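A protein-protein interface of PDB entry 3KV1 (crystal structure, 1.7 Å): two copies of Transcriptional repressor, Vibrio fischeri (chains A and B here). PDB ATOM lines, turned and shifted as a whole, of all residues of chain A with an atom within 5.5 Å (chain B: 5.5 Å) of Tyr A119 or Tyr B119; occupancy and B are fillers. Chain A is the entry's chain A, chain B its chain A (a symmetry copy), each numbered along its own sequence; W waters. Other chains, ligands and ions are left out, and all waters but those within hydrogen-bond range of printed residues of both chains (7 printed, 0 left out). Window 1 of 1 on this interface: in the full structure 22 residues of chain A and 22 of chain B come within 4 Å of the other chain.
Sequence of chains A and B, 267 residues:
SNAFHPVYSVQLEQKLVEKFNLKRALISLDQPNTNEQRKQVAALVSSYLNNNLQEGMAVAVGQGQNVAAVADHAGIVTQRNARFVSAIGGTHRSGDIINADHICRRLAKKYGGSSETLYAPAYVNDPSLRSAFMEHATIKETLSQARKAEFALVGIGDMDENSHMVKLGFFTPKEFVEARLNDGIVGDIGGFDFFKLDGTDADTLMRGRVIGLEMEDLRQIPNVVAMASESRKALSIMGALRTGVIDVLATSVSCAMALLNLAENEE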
ATOM      1  N   GLY A  89     -18.358  25.966 -10.725  1.00  0.00           N
ATOM      2  CA  GLY A  89     -16.973  25.490 -10.831  1.00  0.00           C
ATOM      3  C   GLY A  89     -16.837  23.984 -10.660  1.00  0.00           C
ATOM      4  O   GLY A  89     -17.832  23.263 -10.439  1.00  0.00           O
ATOM      5  N   GLY A  90     -15.600  23.497 -10.711  1.00  0.00           N
ATOM      6  CA  GLY A  90     -15.359  22.065 -10.679  1.00  0.00           C
ATOM      7  C   GLY A  90     -15.119  21.484  -9.307  1.00  0.00           C
ATOM      8  O   GLY A  90     -14.774  22.173  -8.374  1.00  0.00           O
ATOM      9  N   THR A  91     -15.253  20.166  -9.233  1.00  0.00           N
ATOM     10  CA  THR A  91     -15.075  19.432  -7.992  1.00  0.00           C
ATOM     11  C   THR A  91     -13.923  18.434  -8.157  1.00  0.00           C
ATOM     12  O   THR A  91     -13.694  17.943  -9.259  1.00  0.00           O
ATOM     13  CB  THR A  91     -16.377  18.683  -7.664  1.00  0.00           C
ATOM     14  OG1 THR A  91     -16.801  17.957  -8.824  1.00  0.00           O
ATOM     15  CG2 THR A  91     -17.476  19.678  -7.297  1.00  0.00           C
ATOM     16  N   ASN A  99     -19.681  16.712 -11.737  1.00  0.00           N
ATOM     17  CA  ASN A  99     -19.259  18.021 -12.081  1.00  0.00           C
ATOM     18  C   ASN A  99     -20.003  18.653 -13.276  1.00  0.00           C
ATOM     19  O   ASN A  99     -20.148  18.000 -14.232  1.00  0.00           O
ATOM     20  CB  ASN A  99     -17.891  17.668 -12.558  1.00  0.00           C
ATOM     21  CG  ASN A  99     -16.972  18.618 -12.302  1.00  0.00           C
ATOM     22  OD1 ASN A  99     -15.946  18.346 -11.726  1.00  0.00           O
ATOM     23  ND2 ASN A  99     -17.247  19.776 -12.752  1.00  0.00           N
ATOM     24  N   ASP A 101     -18.772  20.602 -15.437  1.00  0.00           N
ATOM     25  CA  ASP A 101     -17.822  20.536 -16.532  1.00  0.00           C
ATOM     26  C   ASP A 101     -17.893  19.170 -17.234  1.00  0.00           C
ATOM     27  O   ASP A 101     -17.938  19.091 -18.476  1.00  0.00           O
ATOM     28  CB  ASP A 101     -16.423  20.803 -15.961  1.00  0.00           C
ATOM     29  CG  ASP A 101     -15.356  20.644 -16.959  1.00  0.00           C
ATOM     30  OD1 ASP A 101     -15.585  21.140 -18.088  1.00  0.00           O
ATOM     31  OD2 ASP A 101     -14.301  20.044 -16.604  1.00  0.00           O
ATOM     32  N   HIS A 102     -17.854  18.085 -16.462  1.00  0.00           N
ATOM     33  CA  HIS A 102     -17.972  16.746 -17.053  1.00  0.00           C
ATOM     34  C   HIS A 102     -19.285  16.587 -17.818  1.00  0.00           C
ATOM     35  O   HIS A 102     -19.298  16.080 -18.932  1.00  0.00           O
ATOM     36  CB  HIS A 102     -17.895  15.660 -15.976  1.00  0.00           C
ATOM     37  CG  HIS A 102     -16.516  15.426 -15.452  1.00  0.00           C
ATOM     38  ND1 HIS A 102     -15.600  14.623 -16.102  1.00  0.00           N
ATOM     39  CD2 HIS A 102     -15.897  15.880 -14.336  1.00  0.00           C
ATOM     40  CE1 HIS A 102     -14.473  14.602 -15.410  1.00  0.00           C
ATOM     41  NE2 HIS A 102     -14.628  15.355 -14.334  1.00  0.00           N
ATOM     42  N   ARG A 105     -19.108  18.383 -21.133  1.00  0.00           N
ATOM     43  CA  ARG A 105     -18.334  17.612 -22.107  1.00  0.00           C
ATOM     44  C   ARG A 105     -19.149  16.474 -22.730  1.00  0.00           C
ATOM     45  O   ARG A 105     -19.083  16.219 -23.946  1.00  0.00           O
ATOM     46  CB  ARG A 105     -17.014  17.102 -21.480  1.00  0.00           C
ATOM     47  CG  ARG A 105     -16.002  18.250 -21.378  1.00  0.00           C
ATOM     48  CD  ARG A 105     -15.087  18.209 -20.150  1.00  0.00           C
ATOM     49  NE  ARG A 105     -14.459  16.920 -19.927  1.00  0.00           N
ATOM     50  CZ  ARG A 105     -13.690  16.641 -18.876  1.00  0.00           C
ATOM     51  NH1 ARG A 105     -13.455  17.568 -17.951  1.00  0.00           N
ATOM     52  NH2 ARG A 105     -13.149  15.434 -18.747  1.00  0.00           N
ATOM     53  N   THR A 117     -15.388  25.474 -20.130  1.00  0.00           N
ATOM     54  CA  THR A 117     -15.131  25.195 -18.705  1.00  0.00           C
ATOM     55  C   THR A 117     -15.075  26.483 -17.869  1.00  0.00           C
ATOM     56  O   THR A 117     -14.593  27.519 -18.347  1.00  0.00           O
ATOM     57  CB  THR A 117     -13.801  24.409 -18.567  1.00  0.00           C
ATOM     58  OG1 THR A 117     -13.976  23.118 -19.169  1.00  0.00           O
ATOM     59  CG2 THR A 117     -13.402  24.235 -17.092  1.00  0.00           C
ATOM     60  N   LEU A 118     -15.606  26.423 -16.645  1.00  0.00           N
ATOM     61  CA  LEU A 118     -15.389  27.504 -15.684  1.00  0.00           C
ATOM     62  C   LEU A 118     -14.127  27.111 -14.922  1.00  0.00           C
ATOM     63  O   LEU A 118     -14.141  26.088 -14.225  1.00  0.00           O
ATOM     64  CB  LEU A 118     -16.610  27.640 -14.759  1.00  0.00           C
ATOM     65  CG  LEU A 118     -16.552  28.801 -13.763  1.00  0.00           C
ATOM     66  CD1 LEU A 118     -16.431  30.157 -14.457  1.00  0.00           C
ATOM     67  CD2 LEU A 118     -17.824  28.759 -12.907  1.00  0.00           C
ATOM     68  N   TYR A 119     -13.020  27.863 -15.108  1.00  0.00           N
ATOM     69  CA  TYR A 119     -11.725  27.516 -14.492  1.00  0.00           C
ATOM     70  C   TYR A 119     -11.608  27.976 -13.042  1.00  0.00           C
ATOM     71  O   TYR A 119     -10.770  28.839 -12.711  1.00  0.00           O
ATOM     72  CB  TYR A 119     -10.549  28.075 -15.340  1.00  0.00           C
ATOM     73  CG  TYR A 119     -10.505  27.400 -16.677  1.00  0.00           C
ATOM     74  CD1 TYR A 119     -10.890  28.080 -17.828  1.00  0.00           C
ATOM     75  CD2 TYR A 119     -10.143  26.059 -16.789  1.00  0.00           C
ATOM     76  CE1 TYR A 119     -10.875  27.443 -19.075  1.00  0.00           C
ATOM     77  CE2 TYR A 119     -10.143  25.408 -18.040  1.00  0.00           C
ATOM     78  CZ  TYR A 119     -10.514  26.112 -19.166  1.00  0.00           C
ATOM     79  OH  TYR A 119     -10.526  25.461 -20.398  1.00  0.00           O
ATOM     80  N   ALA A 120     -12.454  27.407 -12.177  1.00  0.00           N
ATOM     81  CA  ALA A 120     -12.442  27.709 -10.765  1.00  0.00           C
ATOM     82  C   ALA A 120     -13.098  26.528 -10.063  1.00  0.00           C
ATOM     83  O   ALA A 120     -13.931  25.828 -10.659  1.00  0.00           O
ATOM     84  CB  ALA A 120     -13.283  28.948 -10.480  1.00  0.00           C
ATOM     85  N   PRO A 121     -12.755  26.325  -8.799  1.00  0.00           N
ATOM     86  CA  PRO A 121     -13.457  25.252  -8.084  1.00  0.00           C
ATOM     87  C   PRO A 121     -14.919  25.639  -7.783  1.00  0.00           C
ATOM     88  O   PRO A 121     -15.248  26.824  -7.693  1.00  0.00           O
ATOM     89  CB  PRO A 121     -12.708  25.136  -6.746  1.00  0.00           C
ATOM     90  CG  PRO A 121     -11.767  26.265  -6.672  1.00  0.00           C
ATOM     91  CD  PRO A 121     -11.759  27.030  -7.983  1.00  0.00           C
ATOM     92  N   THR A 138     -10.671  35.658 -16.256  1.00  0.00           N
ATOM     93  CA  THR A 138     -10.961  34.392 -16.915  1.00  0.00           C
ATOM     94  C   THR A 138     -12.293  33.787 -16.419  1.00  0.00           C
ATOM     95  O   THR A 138     -13.063  33.218 -17.219  1.00  0.00           O
ATOM     96  CB  THR A 138      -9.826  33.395 -16.681  1.00  0.00           C
ATOM     97  OG1 THR A 138      -8.613  33.952 -17.201  1.00  0.00           O
ATOM     98  CG2 THR A 138     -10.147  32.056 -17.359  1.00  0.00           C
ATOM     99  N   ILE A 139     -12.547  33.918 -15.114  1.00  0.00           N
ATOM    100  CA  ILE A 139     -13.774  33.428 -14.487  1.00  0.00           C
ATOM    101  C   ILE A 139     -14.947  34.311 -14.916  1.00  0.00           C
ATOM    102  O   ILE A 139     -16.000  33.798 -15.290  1.00  0.00           O
ATOM    103  CB  ILE A 139     -13.660  33.370 -12.943  1.00  0.00           C
ATOM    104  CG1 ILE A 139     -12.886  32.130 -12.508  1.00  0.00           C
ATOM    105  CG2 ILE A 139     -15.044  33.254 -12.282  1.00  0.00           C
ATOM    106  CD1 ILE A 139     -11.507  32.135 -12.770  1.00  0.00           C
ATOM    107  N   THR A 142     -16.294  33.505 -18.522  1.00  0.00           N
ATOM    108  CA  THR A 142     -17.124  32.318 -18.679  1.00  0.00           C
ATOM    109  C   THR A 142     -18.483  32.541 -18.029  1.00  0.00           C
ATOM    110  O   THR A 142     -19.512  32.133 -18.570  1.00  0.00           O
ATOM    111  CB  THR A 142     -16.437  31.052 -18.109  1.00  0.00           C
ATOM    112  OG1 THR A 142     -15.227  30.830 -18.845  1.00  0.00           O
ATOM    113  CG2 THR A 142     -17.335  29.824 -18.277  1.00  0.00           C
ATOM    114  N   GLY B  89      -3.290  26.004 -15.695  1.00  0.00           N
ATOM    115  CA  GLY B  89      -4.701  26.410 -15.668  1.00  0.00           C
ATOM    116  C   GLY B  89      -5.224  26.865 -17.022  1.00  0.00           C
ATOM    117  O   GLY B  89      -4.488  26.887 -18.030  1.00  0.00           O
ATOM    118  N   GLY B  90      -6.489  27.279 -17.055  1.00  0.00           N
ATOM    119  CA  GLY B  90      -7.131  27.621 -18.311  1.00  0.00           C
ATOM    120  C   GLY B  90      -7.048  29.078 -18.697  1.00  0.00           C
ATOM    121  O   GLY B  90      -6.820  29.943 -17.882  1.00  0.00           O
ATOM    122  N   THR B  91      -7.307  29.328 -19.975  1.00  0.00           N
ATOM    123  CA  THR B  91      -7.263  30.668 -20.534  1.00  0.00           C
ATOM    124  C   THR B  91      -8.647  31.034 -21.079  1.00  0.00           C
ATOM    125  O   THR B  91      -9.382  30.154 -21.521  1.00  0.00           O
ATOM    126  CB  THR B  91      -6.224  30.701 -21.667  1.00  0.00           C
ATOM    127  OG1 THR B  91      -6.472  29.606 -22.557  1.00  0.00           O
ATOM    128  CG2 THR B  91      -4.818  30.541 -21.094  1.00  0.00           C
ATOM    129  N   ASN B  99      -5.305  26.202 -24.877  1.00  0.00           N
ATOM    130  CA  ASN B  99      -5.396  25.789 -23.523  1.00  0.00           C
ATOM    131  C   ASN B  99      -4.956  24.336 -23.253  1.00  0.00           C
ATOM    132  O   ASN B  99      -5.358  23.505 -23.967  1.00  0.00           O
ATOM    133  CB  ASN B  99      -6.884  25.821 -23.407  1.00  0.00           C
ATOM    134  CG  ASN B  99      -7.318  26.184 -22.187  1.00  0.00           C
ATOM    135  OD1 ASN B  99      -8.113  27.084 -22.056  1.00  0.00           O
ATOM    136  ND2 ASN B  99      -6.875  25.484 -21.221  1.00  0.00           N
ATOM    137  N   ASP B 101      -6.196  22.362 -21.120  1.00  0.00           N
ATOM    138  CA  ASP B 101      -7.437  21.639 -20.913  1.00  0.00           C
ATOM    139  C   ASP B 101      -8.035  21.188 -22.256  1.00  0.00           C
ATOM    140  O   ASP B 101      -8.449  20.024 -22.413  1.00  0.00           O
ATOM    141  CB  ASP B 101      -8.399  22.558 -20.149  1.00  0.00           C
ATOM    142  CG  ASP B 101      -9.738  21.977 -19.984  1.00  0.00           C
ATOM    143  OD1 ASP B 101      -9.773  20.766 -19.660  1.00  0.00           O
ATOM    144  OD2 ASP B 101     -10.735  22.735 -20.162  1.00  0.00           O
ATOM    145  N   HIS B 102      -8.136  22.105 -23.217  1.00  0.00           N
ATOM    146  CA  HIS B 102      -8.646  21.739 -24.544  1.00  0.00           C
ATOM    147  C   HIS B 102      -7.795  20.647 -25.188  1.00  0.00           C
ATOM    148  O   HIS B 102      -8.324  19.684 -25.729  1.00  0.00           O
ATOM    149  CB  HIS B 102      -8.676  22.955 -25.476  1.00  0.00           C
ATOM    150  CG  HIS B 102      -9.791  23.908 -25.191  1.00  0.00           C
ATOM    151  ND1 HIS B 102     -11.073  23.715 -25.662  1.00  0.00           N
ATOM    152  CD2 HIS B 102      -9.814  25.067 -24.491  1.00  0.00           C
ATOM    153  CE1 HIS B 102     -11.841  24.712 -25.255  1.00  0.00           C
ATOM    154  NE2 HIS B 102     -11.100  25.546 -24.545  1.00  0.00           N
ATOM    155  N   ARG B 105      -8.546  17.294 -23.626  1.00  0.00           N
ATOM    156  CA  ARG B 105      -9.805  16.748 -24.133  1.00  0.00           C
ATOM    157  C   ARG B 105      -9.647  16.106 -25.515  1.00  0.00           C
ATOM    158  O   ARG B 105     -10.204  15.029 -25.797  1.00  0.00           O
ATOM    159  CB  ARG B 105     -10.916  17.827 -24.122  1.00  0.00           C
ATOM    160  CG  ARG B 105     -11.426  18.040 -22.690  1.00  0.00           C
ATOM    161  CD  ARG B 105     -11.826  19.479 -22.345  1.00  0.00           C
ATOM    162  NE  ARG B 105     -12.702  20.096 -23.325  1.00  0.00           N
ATOM    163  CZ  ARG B 105     -13.106  21.363 -23.263  1.00  0.00           C
ATOM    164  NH1 ARG B 105     -12.710  22.147 -22.263  1.00  0.00           N
ATOM    165  NH2 ARG B 105     -13.912  21.853 -24.200  1.00  0.00           N
ATOM    166  N   THR B 117      -9.323  18.187 -15.643  1.00  0.00           N
ATOM    167  CA  THR B 117      -9.144  19.648 -15.737  1.00  0.00           C
ATOM    168  C   THR B 117      -8.511  20.232 -14.466  1.00  0.00           C
ATOM    169  O   THR B 117      -8.785  19.759 -13.355  1.00  0.00           O
ATOM    170  CB  THR B 117     -10.518  20.317 -16.007  1.00  0.00           C
ATOM    171  OG1 THR B 117     -10.966  19.916 -17.310  1.00  0.00           O
ATOM    172  CG2 THR B 117     -10.415  21.850 -15.952  1.00  0.00           C
ATOM    173  N   LEU B 118      -7.635  21.226 -14.638  1.00  0.00           N
ATOM    174  CA  LEU B 118      -7.164  22.012 -13.499  1.00  0.00           C
ATOM    175  C   LEU B 118      -8.141  23.179 -13.389  1.00  0.00           C
ATOM    176  O   LEU B 118      -8.201  23.999 -14.314  1.00  0.00           O
ATOM    177  CB  LEU B 118      -5.720  22.481 -13.742  1.00  0.00           C
ATOM    178  CG  LEU B 118      -5.071  23.237 -12.580  1.00  0.00           C
ATOM    179  CD1 LEU B 118      -5.002  22.397 -11.306  1.00  0.00           C
ATOM    180  CD2 LEU B 118      -3.660  23.656 -13.013  1.00  0.00           C
ATOM    181  N   TYR B 119      -8.956  23.218 -12.312  1.00  0.00           N
ATOM    182  CA  TYR B 119      -9.998  24.251 -12.158  1.00  0.00           C
ATOM    183  C   TYR B 119      -9.460  25.568 -11.607  1.00  0.00           C
ATOM    184  O   TYR B 119      -9.823  25.991 -10.491  1.00  0.00           O
ATOM    185  CB  TYR B 119     -11.162  23.724 -11.273  1.00  0.00           C
ATOM    186  CG  TYR B 119     -11.870  22.597 -11.964  1.00  0.00           C
ATOM    187  CD1 TYR B 119     -11.718  21.287 -11.521  1.00  0.00           C
ATOM    188  CD2 TYR B 119     -12.642  22.828 -13.100  1.00  0.00           C
ATOM    189  CE1 TYR B 119     -12.356  20.230 -12.181  1.00  0.00           C
ATOM    190  CE2 TYR B 119     -13.273  21.766 -13.779  1.00  0.00           C
ATOM    191  CZ  TYR B 119     -13.117  20.479 -13.309  1.00  0.00           C
ATOM    192  OH  TYR B 119     -13.732  19.430 -13.990  1.00  0.00           O
ATOM    193  N   ALA B 120      -8.585  26.215 -12.385  1.00  0.00           N
ATOM    194  CA  ALA B 120      -8.015  27.490 -12.020  1.00  0.00           C
ATOM    195  C   ALA B 120      -7.554  28.145 -13.315  1.00  0.00           C
ATOM    196  O   ALA B 120      -7.235  27.448 -14.292  1.00  0.00           O
ATOM    197  CB  ALA B 120      -6.791  27.291 -11.134  1.00  0.00           C
ATOM    198  N   PRO B 121      -7.484  29.468 -13.318  1.00  0.00           N
ATOM    199  CA  PRO B 121      -6.943  30.103 -14.527  1.00  0.00           C
ATOM    200  C   PRO B 121      -5.424  29.871 -14.653  1.00  0.00           C
ATOM    201  O   PRO B 121      -4.737  29.655 -13.651  1.00  0.00           O
ATOM    202  CB  PRO B 121      -7.181  31.605 -14.304  1.00  0.00           C
ATOM    203  CG  PRO B 121      -7.644  31.774 -12.917  1.00  0.00           C
ATOM    204  CD  PRO B 121      -7.869  30.420 -12.270  1.00  0.00           C
ATOM    205  N   THR B 138      -9.044  21.557  -4.261  1.00  0.00           N
ATOM    206  CA  THR B 138      -9.402  21.063  -5.583  1.00  0.00           C
ATOM    207  C   THR B 138      -8.235  21.220  -6.583  1.00  0.00           C
ATOM    208  O   THR B 138      -8.003  20.330  -7.426  1.00  0.00           O
ATOM    209  CB  THR B 138     -10.634  21.797  -6.113  1.00  0.00           C
ATOM    210  OG1 THR B 138     -11.719  21.590  -5.200  1.00  0.00           O
ATOM    211  CG2 THR B 138     -10.994  21.289  -7.515  1.00  0.00           C
ATOM    212  N   ILE B 139      -7.519  22.343  -6.477  1.00  0.00           N
ATOM    213  CA  ILE B 139      -6.365  22.636  -7.325  1.00  0.00           C
ATOM    214  C   ILE B 139      -5.201  21.726  -6.927  1.00  0.00           C
ATOM    215  O   ILE B 139      -4.554  21.139  -7.792  1.00  0.00           O
ATOM    216  CB  ILE B 139      -5.950  24.128  -7.256  1.00  0.00           C
ATOM    217  CG1 ILE B 139      -6.867  24.980  -8.127  1.00  0.00           C
ATOM    218  CG2 ILE B 139      -4.530  24.342  -7.807  1.00  0.00           C
ATOM    219  CD1 ILE B 139      -8.179  25.157  -7.660  1.00  0.00           C
ATOM    220  N   THR B 142      -5.500  18.069  -8.344  1.00  0.00           N
ATOM    221  CA  THR B 142      -5.182  17.867  -9.751  1.00  0.00           C
ATOM    222  C   THR B 142      -3.684  18.021  -9.975  1.00  0.00           C
ATOM    223  O   THR B 142      -3.083  17.267 -10.743  1.00  0.00           O
ATOM    224  CB  THR B 142      -5.983  18.824 -10.668  1.00  0.00           C
ATOM    225  OG1 THR B 142      -7.379  18.542 -10.498  1.00  0.00           O
ATOM    226  CG2 THR B 142      -5.621  18.597 -12.138  1.00  0.00           C
HETATM  227  O   HOH W   1     -12.786  20.667 -19.194  1.00  0.00           O
HETATM  228  O   HOH W   2      -5.971  32.759 -17.404  1.00  0.00           O
HETATM  229  O   HOH W   3     -13.103  25.932 -21.860  1.00  0.00           O
HETATM  230  O   HOH W   4     -11.806  17.191 -14.518  1.00  0.00           O
HETATM  231  O   HOH W   5     -14.498  22.410  -5.416  1.00  0.00           O
HETATM  232  O   HOH W   6     -10.513  18.249 -19.292  1.00  0.00           O
HETATM  233  O   HOH W   7     -15.574  21.679 -20.682  1.00  0.00           O
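N of Gly A90 sits at hydrogen-bond distance from O of Ala A120, 2.9 Å away. OG1 of Thr A91 lies within hydrogen-bond range of OD1 of Asn A99, at 3.1 Å. OD2 of Asp A101 is in salt-bridge range of NH1 of Arg A105 (2.9 Å). The side-chain carboxylate (OD1) of Asp A101 is in hydrogen-bond range of the side-chain hydroxyl (OG1) of Thr A117. N of Gly B90 is in hydrogen-bond range of O of Ala B120, at 2.9 Å. The side-chain hydroxyl of Thr B91 is in hydrogen-bond range of the side-chain amide oxygen of Asn B99, at 3.1 Å.
OH of Tyr B119 sits at hydrogen-bond distance from OD1 of Asn A99. OD2 of Asp A101 sits at hydrogen-bond distance from OG1 of Thr B117 (3.4 Å). The side-chain carboxylate of Asp A101 is in hydrogen-bond range of the side-chain hydroxyl of Tyr B119 (2.7 Å). The side-chain hydroxyl (OG1) of Thr B117 lies within hydrogen-bond range of the guanidinium group (NH1) of Arg A105 (3.5 Å). The side-chain hydroxyl (OG1) of Thr A117 is in hydrogen-bond range of the side-chain carboxylate (OD2) of Asp B101, 3.4 Å away. NH1 of Arg B105 sits at hydrogen-bond distance from OG1 of Thr A117, at 3.5 Å. OH of Tyr A119 lies within hydrogen-bond range of OD1 of Asn B99, 3.3 Å away. OH of Tyr A119 is in hydrogen-bond range of OD2 of Asp B101 (2.7 Å). The backbone NH (N) of Ala B120 sits close to the backbone carbonyl oxygen (O) of Tyr A119 (3.4 Å). The backbone NH (N) of Ala A120 lies close to the backbone carbonyl oxygen (O) of Tyr B119 (3.4 Å). The backbone nitrogen (N) of Pro B121 lies close to the backbone carbonyl oxygen (O) of Tyr A119 (3.4 Å). The backbone nitrogen (N) of Pro A121 sits close to the backbone carbonyl oxygen (O) of Tyr B119, 3.4 Å away.
Water W7 lies within hydrogen-bond range of OG1 of Thr A117 (2.6 Å), OD1 of Asp A101 (2.6 Å) and NH1 of Arg B105 (3.3 Å). Water W6 lies within hydrogen-bond range of OG1 of Thr B117 (2.6 Å), OD1 of Asp B101 (2.6 Å) and NH1 of Arg A105 (3.3 Å). Water W1 lies within hydrogen-bond range of the side-chain hydroxyl (OG1) of Thr A117, the side-chain hydroxyl (OG1) of Thr B117, the side-chain carboxylate (OD1) of Asp A101, the side-chain carboxylate (OD1) of Asp B101, the guanidinium group (NH1) of Arg A105 and the guanidinium group (NH1) of Arg B105. Water W3 lies within hydrogen-bond range of N of Thr A117, OH of Tyr A119 and NE2 of His B102. Water W2 lies within hydrogen-bond range of the side-chain hydroxyl of Thr A138 (2.9 Å) and the backbone carbonyl oxygen of Gly B90 (3.0 Å). Water W5 bridges the side-chain hydroxyl of Thr B138 (2.9 Å) and the backbone carbonyl oxygen of Gly A90 (3.0 Å).
Of the printed residues of chain B, Thr A91 touches Tyr B119 (3.9 Å). Of the printed residues of chain B, Tyr A119 touches Gly B90, Thr B91, Asn B99, Asp B101, Leu B118, Tyr B119, Ala B120 and Pro B121. Printed residues of chain B within 4 Å of Ala A120: Tyr B119 (3.1 Å). Of the printed residues of chain A, Leu B118 touches Tyr A119. Of the printed residues of chain A, Tyr B119 touches Gly A90, Thr A91, Asn A99, Asp A101, Leu A118, Tyr A119, Ala A120 and Pro A121. Printed residues of chain A within 4 Å of Pro B121: Tyr A119, Thr A138 and Ile A139. Of the printed residues of chain A, Ile B139 touches Pro A121. The nearest printed residue of chain A that does not touch Tyr B119 is Thr A117 (4.1 Å). The nearest printed residue of chain B that does not touch Leu A118 is Ala B120 (5.9 Å).
Gly A90 touches Thr B138, and with the chains exchanged Thr A138 touches Gly B90. Thr A91 touches Tyr B119, and with the chains exchanged Tyr A119 touches Thr B91. Tyr A119 touches Ala B120, and with the chains exchanged Ala A120 touches Tyr B119. Pro A121 touches Thr B138, and with the chains exchanged Thr A138 touches Pro B121. Positions printed for both chains: 89, 90, 91, 99, 101, 102, 105, 117, 118, 119, 120, 121, 138, 139 and 142. Of the 26 pairs that touch across the chains among the printed residues, 26 have their exchanged pair printed and touching as well.
Of the 15 printed residues of chain A, 12 touch a printed residue of chain B. Printed residues of chain A that touch a printed residue of chain B: Gly A90, Thr A91, Asn A99, Asp A101, Arg A105, Thr A117, Leu A118, Tyr A119, Ala A120, Pro A121, Thr A138 and Ile A139. Hydrophobic or aromatic side chains of chain A that line the printed part of chain B: Tyr A119, Pro A121 and Ile A139. Of the 15 printed residues of chain B, 12 touch a printed residue of chain A. Printed residues of chain B that touch a printed residue of chain A: Gly B90, Thr B91, Asn B99, Asp B101, Arg B105, Thr B117, Leu B118, Tyr B119, Ala B120, Pro B121, Thr B138 and Ile B139. Hydrophobic or aromatic side chains of chain B within 4 Å of the printed part of chain A: Tyr B119, Pro B121 and Ile B139. Along chain B the printed residues that touch a printed residue of chain A span positions 90 to 139.
Gly A90 touches Tyr B119 (CA to CD2, 3.7 Å). CG2 of Thr B138 touches O of Gly A90 (3.98 Å). Thr B117 touches Thr A117. Tyr B119 touches Leu A118. CD2 of Tyr A119 touches CA of Gly B90, at 3.7 Å. Thr B91 touches Tyr A119. Tyr A119 touches Leu B118. CB of Thr B138 touches CB of Pro A121, 3.98 Å away. CG2 of Thr A138 touches O of Gly B90, at 3.98 Å. Pro B121 touches Thr A138.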
